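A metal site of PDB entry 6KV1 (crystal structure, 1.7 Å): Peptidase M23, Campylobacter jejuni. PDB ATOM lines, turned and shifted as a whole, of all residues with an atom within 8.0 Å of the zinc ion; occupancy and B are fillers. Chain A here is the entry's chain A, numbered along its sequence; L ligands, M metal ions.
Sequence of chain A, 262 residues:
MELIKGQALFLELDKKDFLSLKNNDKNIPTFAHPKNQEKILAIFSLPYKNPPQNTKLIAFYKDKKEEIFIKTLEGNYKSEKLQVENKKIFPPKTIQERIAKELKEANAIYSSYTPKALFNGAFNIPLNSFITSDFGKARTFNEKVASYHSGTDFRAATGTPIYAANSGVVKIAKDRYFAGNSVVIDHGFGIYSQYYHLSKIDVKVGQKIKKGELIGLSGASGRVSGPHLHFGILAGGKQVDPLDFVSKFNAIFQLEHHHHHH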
ATOM      1  N   GLU A  80      11.672  -4.122 -19.825  1.00  0.00           N
ATOM      2  CA  GLU A  80      10.287  -4.151 -20.275  1.00  0.00           C
ATOM      3  C   GLU A  80       9.363  -4.107 -19.055  1.00  0.00           C
ATOM      4  O   GLU A  80       9.765  -4.456 -17.946  1.00  0.00           O
ATOM      5  CB  GLU A  80       9.995  -5.377 -21.156  1.00  0.00           C
ATOM      6  CG  GLU A  80       9.700  -6.685 -20.431  1.00  0.00           C
ATOM      7  CD  GLU A  80       9.319  -7.817 -21.385  1.00  0.00           C
ATOM      8  OE1 GLU A  80       9.211  -7.576 -22.601  1.00  0.00           O
ATOM      9  OE2 GLU A  80       9.134  -8.966 -20.928  1.00  0.00           O
ATOM     10  N   LEU A  82       5.489  -5.162 -17.501  1.00  0.00           N
ATOM     11  CA  LEU A  82       4.443  -6.157 -17.684  1.00  0.00           C
ATOM     12  C   LEU A  82       3.385  -6.018 -16.602  1.00  0.00           C
ATOM     13  O   LEU A  82       3.696  -5.804 -15.429  1.00  0.00           O
ATOM     14  CB  LEU A  82       5.012  -7.576 -17.639  1.00  0.00           C
ATOM     15  CG  LEU A  82       5.795  -7.988 -18.894  1.00  0.00           C
ATOM     16  CD1 LEU A  82       6.200  -9.434 -18.786  1.00  0.00           C
ATOM     17  CD2 LEU A  82       4.933  -7.759 -20.113  1.00  0.00           C
ATOM     18  N   THR A 132       7.930 -12.698 -29.045  1.00  0.00           N
ATOM     19  CA  THR A 132       7.249 -11.564 -28.452  1.00  0.00           C
ATOM     20  C   THR A 132       7.977 -11.001 -27.246  1.00  0.00           C
ATOM     21  O   THR A 132       7.750  -9.846 -26.890  1.00  0.00           O
ATOM     22  CB  THR A 132       5.830 -11.956 -28.021  1.00  0.00           C
ATOM     23  OG1 THR A 132       5.905 -13.067 -27.123  1.00  0.00           O
ATOM     24  CG2 THR A 132       5.004 -12.370 -29.230  1.00  0.00           C
ATOM     25  N   SER A 133       8.824 -11.787 -26.597  1.00  0.00           N
ATOM     26  CA  SER A 133       9.556 -11.291 -25.435  1.00  0.00           C
ATOM     27  C   SER A 133      10.821 -12.126 -25.325  1.00  0.00           C
ATOM     28  O   SER A 133      10.756 -13.325 -25.002  1.00  0.00           O
ATOM     29  CB  SER A 133       8.709 -11.384 -24.178  1.00  0.00           C
ATOM     30  OG  SER A 133       9.427 -10.933 -23.052  1.00  0.00           O
ATOM     31  N   ASP A 134      11.956 -11.508 -25.616  1.00  0.00           N
ATOM     32  CA  ASP A 134      13.221 -12.233 -25.740  1.00  0.00           C
ATOM     33  C   ASP A 134      13.798 -12.570 -24.365  1.00  0.00           C
ATOM     34  O   ASP A 134      13.359 -12.070 -23.318  1.00  0.00           O
ATOM     35  CB  ASP A 134      14.209 -11.390 -26.557  1.00  0.00           C
ATOM     36  CG  ASP A 134      15.110 -12.250 -27.441  1.00  0.00           C
ATOM     37  OD1 ASP A 134      15.164 -13.476 -27.217  1.00  0.00           O
ATOM     38  OD2 ASP A 134      15.780 -11.690 -28.340  1.00  0.00           O
ATOM     39  N   PHE A 135      14.794 -13.459 -24.373  1.00  0.00           N
ATOM     40  CA  PHE A 135      15.445 -13.867 -23.135  1.00  0.00           C
ATOM     41  C   PHE A 135      16.186 -12.707 -22.470  1.00  0.00           C
ATOM     42  O   PHE A 135      16.755 -11.844 -23.140  1.00  0.00           O
ATOM     43  CB  PHE A 135      16.436 -15.005 -23.406  1.00  0.00           C
ATOM     44  CG  PHE A 135      17.214 -15.417 -22.201  1.00  0.00           C
ATOM     45  CD1 PHE A 135      16.742 -16.405 -21.362  1.00  0.00           C
ATOM     46  CD2 PHE A 135      18.447 -14.833 -21.908  1.00  0.00           C
ATOM     47  CE1 PHE A 135      17.457 -16.806 -20.253  1.00  0.00           C
ATOM     48  CE2 PHE A 135      19.168 -15.228 -20.780  1.00  0.00           C
ATOM     49  CZ  PHE A 135      18.679 -16.215 -19.970  1.00  0.00           C
ATOM     50  N   ARG A 139      12.742  -7.068 -16.277  1.00  0.00           N
ATOM     51  CA  ARG A 139      11.306  -6.836 -16.215  1.00  0.00           C
ATOM     52  C   ARG A 139      10.923  -6.074 -14.956  1.00  0.00           C
ATOM     53  O   ARG A 139      11.628  -6.093 -13.939  1.00  0.00           O
ATOM     54  CB  ARG A 139      10.534  -8.162 -16.260  1.00  0.00           C
ATOM     55  CG  ARG A 139      10.770  -8.915 -17.538  1.00  0.00           C
ATOM     56  CD  ARG A 139      10.093 -10.272 -17.511  1.00  0.00           C
ATOM     57  NE  ARG A 139       9.646 -10.635 -18.848  1.00  0.00           N
ATOM     58  CZ  ARG A 139       9.060 -11.782 -19.156  1.00  0.00           C
ATOM     59  NH1 ARG A 139       8.856 -12.691 -18.219  1.00  0.00           N
ATOM     60  NH2 ARG A 139       8.669 -12.008 -20.401  1.00  0.00           N
ATOM     61  N   TYR A 148      13.559 -10.847 -14.123  1.00  0.00           N
ATOM     62  CA  TYR A 148      14.218 -11.002 -15.409  1.00  0.00           C
ATOM     63  C   TYR A 148      13.565 -12.156 -16.143  1.00  0.00           C
ATOM     64  O   TYR A 148      13.009 -13.070 -15.525  1.00  0.00           O
ATOM     65  CB  TYR A 148      15.727 -11.232 -15.242  1.00  0.00           C
ATOM     66  CG  TYR A 148      16.149 -12.687 -15.190  1.00  0.00           C
ATOM     67  CD1 TYR A 148      16.118 -13.397 -13.997  1.00  0.00           C
ATOM     68  CD2 TYR A 148      16.602 -13.355 -16.325  1.00  0.00           C
ATOM     69  CE1 TYR A 148      16.495 -14.729 -13.931  1.00  0.00           C
ATOM     70  CE2 TYR A 148      16.983 -14.694 -16.280  1.00  0.00           C
ATOM     71  CZ  TYR A 148      16.939 -15.368 -15.074  1.00  0.00           C
ATOM     72  OH  TYR A 148      17.320 -16.693 -14.990  1.00  0.00           O
ATOM     73  N   HIS A 149      13.635 -12.121 -17.478  1.00  0.00           N
ATOM     74  CA  HIS A 149      13.016 -13.140 -18.310  1.00  0.00           C
ATOM     75  C   HIS A 149      13.964 -14.316 -18.480  1.00  0.00           C
ATOM     76  O   HIS A 149      15.006 -14.188 -19.125  1.00  0.00           O
ATOM     77  CB  HIS A 149      12.642 -12.563 -19.677  1.00  0.00           C
ATOM     78  CG  HIS A 149      11.693 -13.432 -20.439  1.00  0.00           C
ATOM     79  ND1 HIS A 149      11.408 -13.239 -21.778  1.00  0.00           N
ATOM     80  CD2 HIS A 149      10.953 -14.506 -20.056  1.00  0.00           C
ATOM     81  CE1 HIS A 149      10.556 -14.150 -22.192  1.00  0.00           C
ATOM     82  NE2 HIS A 149      10.252 -14.930 -21.164  1.00  0.00           N
ATOM     83  N   SER A 150      13.579 -15.475 -17.945  1.00  0.00           N
ATOM     84  CA  SER A 150      14.431 -16.659 -17.902  1.00  0.00           C
ATOM     85  C   SER A 150      14.160 -17.634 -19.036  1.00  0.00           C
ATOM     86  O   SER A 150      14.678 -18.760 -19.034  1.00  0.00           O
ATOM     87  CB  SER A 150      14.292 -17.374 -16.548  1.00  0.00           C
ATOM     88  OG  SER A 150      12.965 -17.841 -16.356  1.00  0.00           O
ATOM     89  N   GLY A 151      13.331 -17.245 -20.003  1.00  0.00           N
ATOM     90  CA  GLY A 151      13.147 -17.989 -21.227  1.00  0.00           C
ATOM     91  C   GLY A 151      12.814 -17.055 -22.356  1.00  0.00           C
ATOM     92  O   GLY A 151      13.115 -15.855 -22.285  1.00  0.00           O
ATOM     93  N   THR A 152      12.208 -17.571 -23.414  1.00  0.00           N
ATOM     94  CA  THR A 152      11.799 -16.754 -24.549  1.00  0.00           C
ATOM     95  C   THR A 152      10.332 -17.015 -24.845  1.00  0.00           C
ATOM     96  O   THR A 152       9.879 -18.169 -24.794  1.00  0.00           O
ATOM     97  CB  THR A 152      12.680 -17.049 -25.792  1.00  0.00           C
ATOM     98  OG1 THR A 152      12.361 -16.136 -26.853  1.00  0.00           O
ATOM     99  CG2 THR A 152      12.495 -18.492 -26.281  1.00  0.00           C
ATOM    100  N   ASP A 153       9.576 -15.936 -25.095  1.00  0.00           N
ATOM    101  CA  ASP A 153       8.137 -16.033 -25.345  1.00  0.00           C
ATOM    102  C   ASP A 153       7.864 -15.978 -26.837  1.00  0.00           C
ATOM    103  O   ASP A 153       8.412 -15.128 -27.550  1.00  0.00           O
ATOM    104  CB  ASP A 153       7.402 -14.898 -24.630  1.00  0.00           C
ATOM    105  CG  ASP A 153       7.461 -15.048 -23.126  1.00  0.00           C
ATOM    106  OD1 ASP A 153       7.737 -16.185 -22.687  1.00  0.00           O
ATOM    107  OD2 ASP A 153       7.256 -14.038 -22.422  1.00  0.00           O
ATOM    108  N   PHE A 154       7.000 -16.885 -27.303  1.00  0.00           N
ATOM    109  CA  PHE A 154       6.554 -16.937 -28.691  1.00  0.00           C
ATOM    110  C   PHE A 154       5.092 -16.552 -28.771  1.00  0.00           C
ATOM    111  O   PHE A 154       4.306 -16.903 -27.890  1.00  0.00           O
ATOM    112  CB  PHE A 154       6.711 -18.341 -29.282  1.00  0.00           C
ATOM    113  CG  PHE A 154       8.133 -18.757 -29.540  1.00  0.00           C
ATOM    114  CD1 PHE A 154       8.907 -19.277 -28.526  1.00  0.00           C
ATOM    115  CD2 PHE A 154       8.686 -18.624 -30.797  1.00  0.00           C
ATOM    116  CE1 PHE A 154      10.204 -19.660 -28.762  1.00  0.00           C
ATOM    117  CE2 PHE A 154       9.978 -19.004 -31.055  1.00  0.00           C
ATOM    118  CZ  PHE A 154      10.745 -19.520 -30.029  1.00  0.00           C
ATOM    119  N   TYR A 196       5.841 -23.603 -20.853  1.00  0.00           N
ATOM    120  CA  TYR A 196       5.020 -23.088 -19.765  1.00  0.00           C
ATOM    121  C   TYR A 196       3.758 -22.423 -20.275  1.00  0.00           C
ATOM    122  O   TYR A 196       3.629 -22.084 -21.453  1.00  0.00           O
ATOM    123  CB  TYR A 196       5.789 -22.084 -18.903  1.00  0.00           C
ATOM    124  CG  TYR A 196       6.977 -22.648 -18.135  1.00  0.00           C
ATOM    125  CD1 TYR A 196       7.194 -24.023 -18.024  1.00  0.00           C
ATOM    126  CD2 TYR A 196       7.904 -21.786 -17.550  1.00  0.00           C
ATOM    127  CE1 TYR A 196       8.292 -24.512 -17.323  1.00  0.00           C
ATOM    128  CE2 TYR A 196       8.997 -22.272 -16.871  1.00  0.00           C
ATOM    129  CZ  TYR A 196       9.186 -23.634 -16.756  1.00  0.00           C
ATOM    130  OH  TYR A 196      10.272 -24.097 -16.072  1.00  0.00           O
ATOM    131  N   HIS A 197       2.829 -22.230 -19.332  1.00  0.00           N
ATOM    132  CA  HIS A 197       1.558 -21.519 -19.496  1.00  0.00           C
ATOM    133  C   HIS A 197       0.603 -22.232 -20.450  1.00  0.00           C
ATOM    134  O   HIS A 197      -0.293 -21.615 -21.008  1.00  0.00           O
ATOM    135  CB  HIS A 197       1.765 -20.073 -19.950  1.00  0.00           C
ATOM    136  CG  HIS A 197       2.826 -19.368 -19.163  1.00  0.00           C
ATOM    137  ND1 HIS A 197       2.732 -19.184 -17.808  1.00  0.00           N
ATOM    138  CD2 HIS A 197       4.012 -18.836 -19.547  1.00  0.00           C
ATOM    139  CE1 HIS A 197       3.817 -18.557 -17.370  1.00  0.00           C
ATOM    140  NE2 HIS A 197       4.606 -18.333 -18.405  1.00  0.00           N
ATOM    141  N   ARG A 223       1.372 -17.210 -14.218  1.00  0.00           N
ATOM    142  CA  ARG A 223       1.611 -15.776 -14.209  1.00  0.00           C
ATOM    143  C   ARG A 223       1.820 -15.302 -15.642  1.00  0.00           C
ATOM    144  O   ARG A 223       2.873 -15.549 -16.240  1.00  0.00           O
ATOM    145  CB  ARG A 223       2.826 -15.437 -13.339  1.00  0.00           C
ATOM    146  CG  ARG A 223       3.258 -13.983 -13.442  1.00  0.00           C
ATOM    147  CD  ARG A 223       4.241 -13.630 -12.331  1.00  0.00           C
ATOM    148  NE  ARG A 223       5.502 -14.342 -12.479  1.00  0.00           N
ATOM    149  CZ  ARG A 223       6.364 -14.556 -11.493  1.00  0.00           C
ATOM    150  NH1 ARG A 223       6.094 -14.115 -10.265  1.00  0.00           N
ATOM    151  NH2 ARG A 223       7.487 -15.202 -11.736  1.00  0.00           N
ATOM    152  N   HIS A 228       0.457 -16.880 -24.431  1.00  0.00           N
ATOM    153  CA  HIS A 228       1.677 -17.056 -25.239  1.00  0.00           C
ATOM    154  C   HIS A 228       2.274 -18.399 -24.880  1.00  0.00           C
ATOM    155  O   HIS A 228       1.826 -19.080 -23.945  1.00  0.00           O
ATOM    156  CB  HIS A 228       2.690 -15.932 -24.993  1.00  0.00           C
ATOM    157  CG  HIS A 228       3.136 -15.867 -23.567  1.00  0.00           C
ATOM    158  ND1 HIS A 228       2.371 -15.293 -22.578  1.00  0.00           N
ATOM    159  CD2 HIS A 228       4.243 -16.365 -22.952  1.00  0.00           C
ATOM    160  CE1 HIS A 228       2.994 -15.419 -21.417  1.00  0.00           C
ATOM    161  NE2 HIS A 228       4.129 -16.059 -21.611  1.00  0.00           N
ATOM    162  N   LEU A 229       3.325 -18.785 -25.604  1.00  0.00           N
ATOM    163  CA  LEU A 229       4.149 -19.922 -25.211  1.00  0.00           C
ATOM    164  C   LEU A 229       5.453 -19.398 -24.623  1.00  0.00           C
ATOM    165  O   LEU A 229       6.057 -18.472 -25.171  1.00  0.00           O
ATOM    166  CB  LEU A 229       4.429 -20.863 -26.383  1.00  0.00           C
ATOM    167  CG  LEU A 229       5.500 -21.915 -26.030  1.00  0.00           C
ATOM    168  CD1 LEU A 229       4.905 -23.109 -25.275  1.00  0.00           C
ATOM    169  CD2 LEU A 229       6.262 -22.382 -27.260  1.00  0.00           C
ATOM    170  N   HIS A 230       5.856 -19.964 -23.496  1.00  0.00           N
ATOM    171  CA  HIS A 230       7.154 -19.684 -22.911  1.00  0.00           C
ATOM    172  C   HIS A 230       8.014 -20.915 -23.126  1.00  0.00           C
ATOM    173  O   HIS A 230       7.606 -22.027 -22.764  1.00  0.00           O
ATOM    174  CB  HIS A 230       7.023 -19.351 -21.432  1.00  0.00           C
ATOM    175  CG  HIS A 230       8.330 -19.333 -20.686  1.00  0.00           C
ATOM    176  ND1 HIS A 230       8.932 -18.170 -20.268  1.00  0.00           N
ATOM    177  CD2 HIS A 230       9.115 -20.338 -20.250  1.00  0.00           C
ATOM    178  CE1 HIS A 230      10.050 -18.456 -19.619  1.00  0.00           C
ATOM    179  NE2 HIS A 230      10.182 -19.773 -19.592  1.00  0.00           N
ATOM    180  N   PHE A 231       9.167 -20.735 -23.764  1.00  0.00           N
ATOM    181  CA  PHE A 231      10.102 -21.810 -24.041  1.00  0.00           C
ATOM    182  C   PHE A 231      11.371 -21.536 -23.262  1.00  0.00           C
ATOM    183  O   PHE A 231      11.872 -20.402 -23.276  1.00  0.00           O
ATOM    184  CB  PHE A 231      10.398 -21.902 -25.546  1.00  0.00           C
ATOM    185  CG  PHE A 231      11.354 -23.013 -25.893  1.00  0.00           C
ATOM    186  CD1 PHE A 231      11.012 -24.324 -25.644  1.00  0.00           C
ATOM    187  CD2 PHE A 231      12.596 -22.735 -26.457  1.00  0.00           C
ATOM    188  CE1 PHE A 231      11.875 -25.350 -25.941  1.00  0.00           C
ATOM    189  CE2 PHE A 231      13.469 -23.753 -26.759  1.00  0.00           C
ATOM    190  CZ  PHE A 231      13.108 -25.062 -26.505  1.00  0.00           C
ATOM    191  N   GLY A 232      11.892 -22.554 -22.579  1.00  0.00           N
ATOM    192  CA  GLY A 232      13.081 -22.389 -21.785  1.00  0.00           C
ATOM    193  C   GLY A 232      14.022 -23.561 -21.944  1.00  0.00           C
ATOM    194  O   GLY A 232      13.625 -24.668 -22.304  1.00  0.00           O
HETATM  195  C1  LIG L   1       5.957 -15.693 -16.398  1.00  0.00           C
HETATM  196  O1  LIG L   1       6.280 -16.773 -16.958  1.00  0.00           O
HETATM  197  O2  LIG L   1       5.706 -15.741 -15.174  1.00  0.00           O
HETATM  198  C2  LIG L   1       5.853 -14.354 -17.126  1.00  0.00           C
HETATM  199  C3  LIG L   1       5.484 -14.450 -18.606  1.00  0.00           C
HETATM  200  O3  LIG L   1       4.154 -15.023 -18.692  1.00  0.00           O
HETATM  201  C4  LIG L   1       5.489 -13.096 -19.313  1.00  0.00           C
HETATM  202  C5  LIG L   1       4.158 -12.388 -19.243  1.00  0.00           C
HETATM  203  O4  LIG L   1       3.600 -11.983 -20.297  1.00  0.00           O
HETATM  204  O5  LIG L   1       3.594 -12.195 -18.146  1.00  0.00           O
HETATM  205  C6  LIG L   1       6.485 -15.336 -19.312  1.00  0.00           C
HETATM  206  O6  LIG L   1       7.700 -15.116 -19.153  1.00  0.00           O
HETATM  207  O7  LIG L   1       6.123 -16.309 -19.988  1.00  0.00           O
HETATM  208 ZN    ZN M   1       8.487 -16.162 -20.772  1.00  0.00          ZN
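The guanidinium group (NH2) of Arg 139 is in salt-bridge range of the side-chain carboxylate (OD2) of Asp 153, 3.2 Å away. The backbone carbonyl oxygen of Ser 133 sits at hydrogen-bond distance from the backbone NH of Asp 153 (2.9 Å). N of Thr 132 sits at hydrogen-bond distance from O of Asp 153 (2.9 Å). O of His 230 sits at hydrogen-bond distance from N of Tyr 196. ND1 of His 149 lies within hydrogen-bond range of NH2 of Arg 139 (3.3 Å). ND1 of His 149 sits close to O of Gly 151. ND1 of His 149 sits close to O of Ser 133. The backbone carbonyl oxygen of Asp 134 lies within hydrogen-bond range of a ring nitrogen (ND1) of His 149, at 2.7 Å.
Of the 22 residues printed, 3 come within 4 Å of the zinc ion. The nearest printed residue that does not touch the zinc ion is Arg 139 (4.2 Å).
The zinc ion is bound by the side-chain carboxylate (OD1) of Asp 153 (2.1 Å), an oxygen (O6) of the ligand (2.1 Å), a ring nitrogen (ND1) of His 230 (2.1 Å), a ring nitrogen (NE2) of His 149 (2.2 Å) and an oxygen (O7) of the ligand (2.5 Å). The zinc ion has five donor atoms within binding distance.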
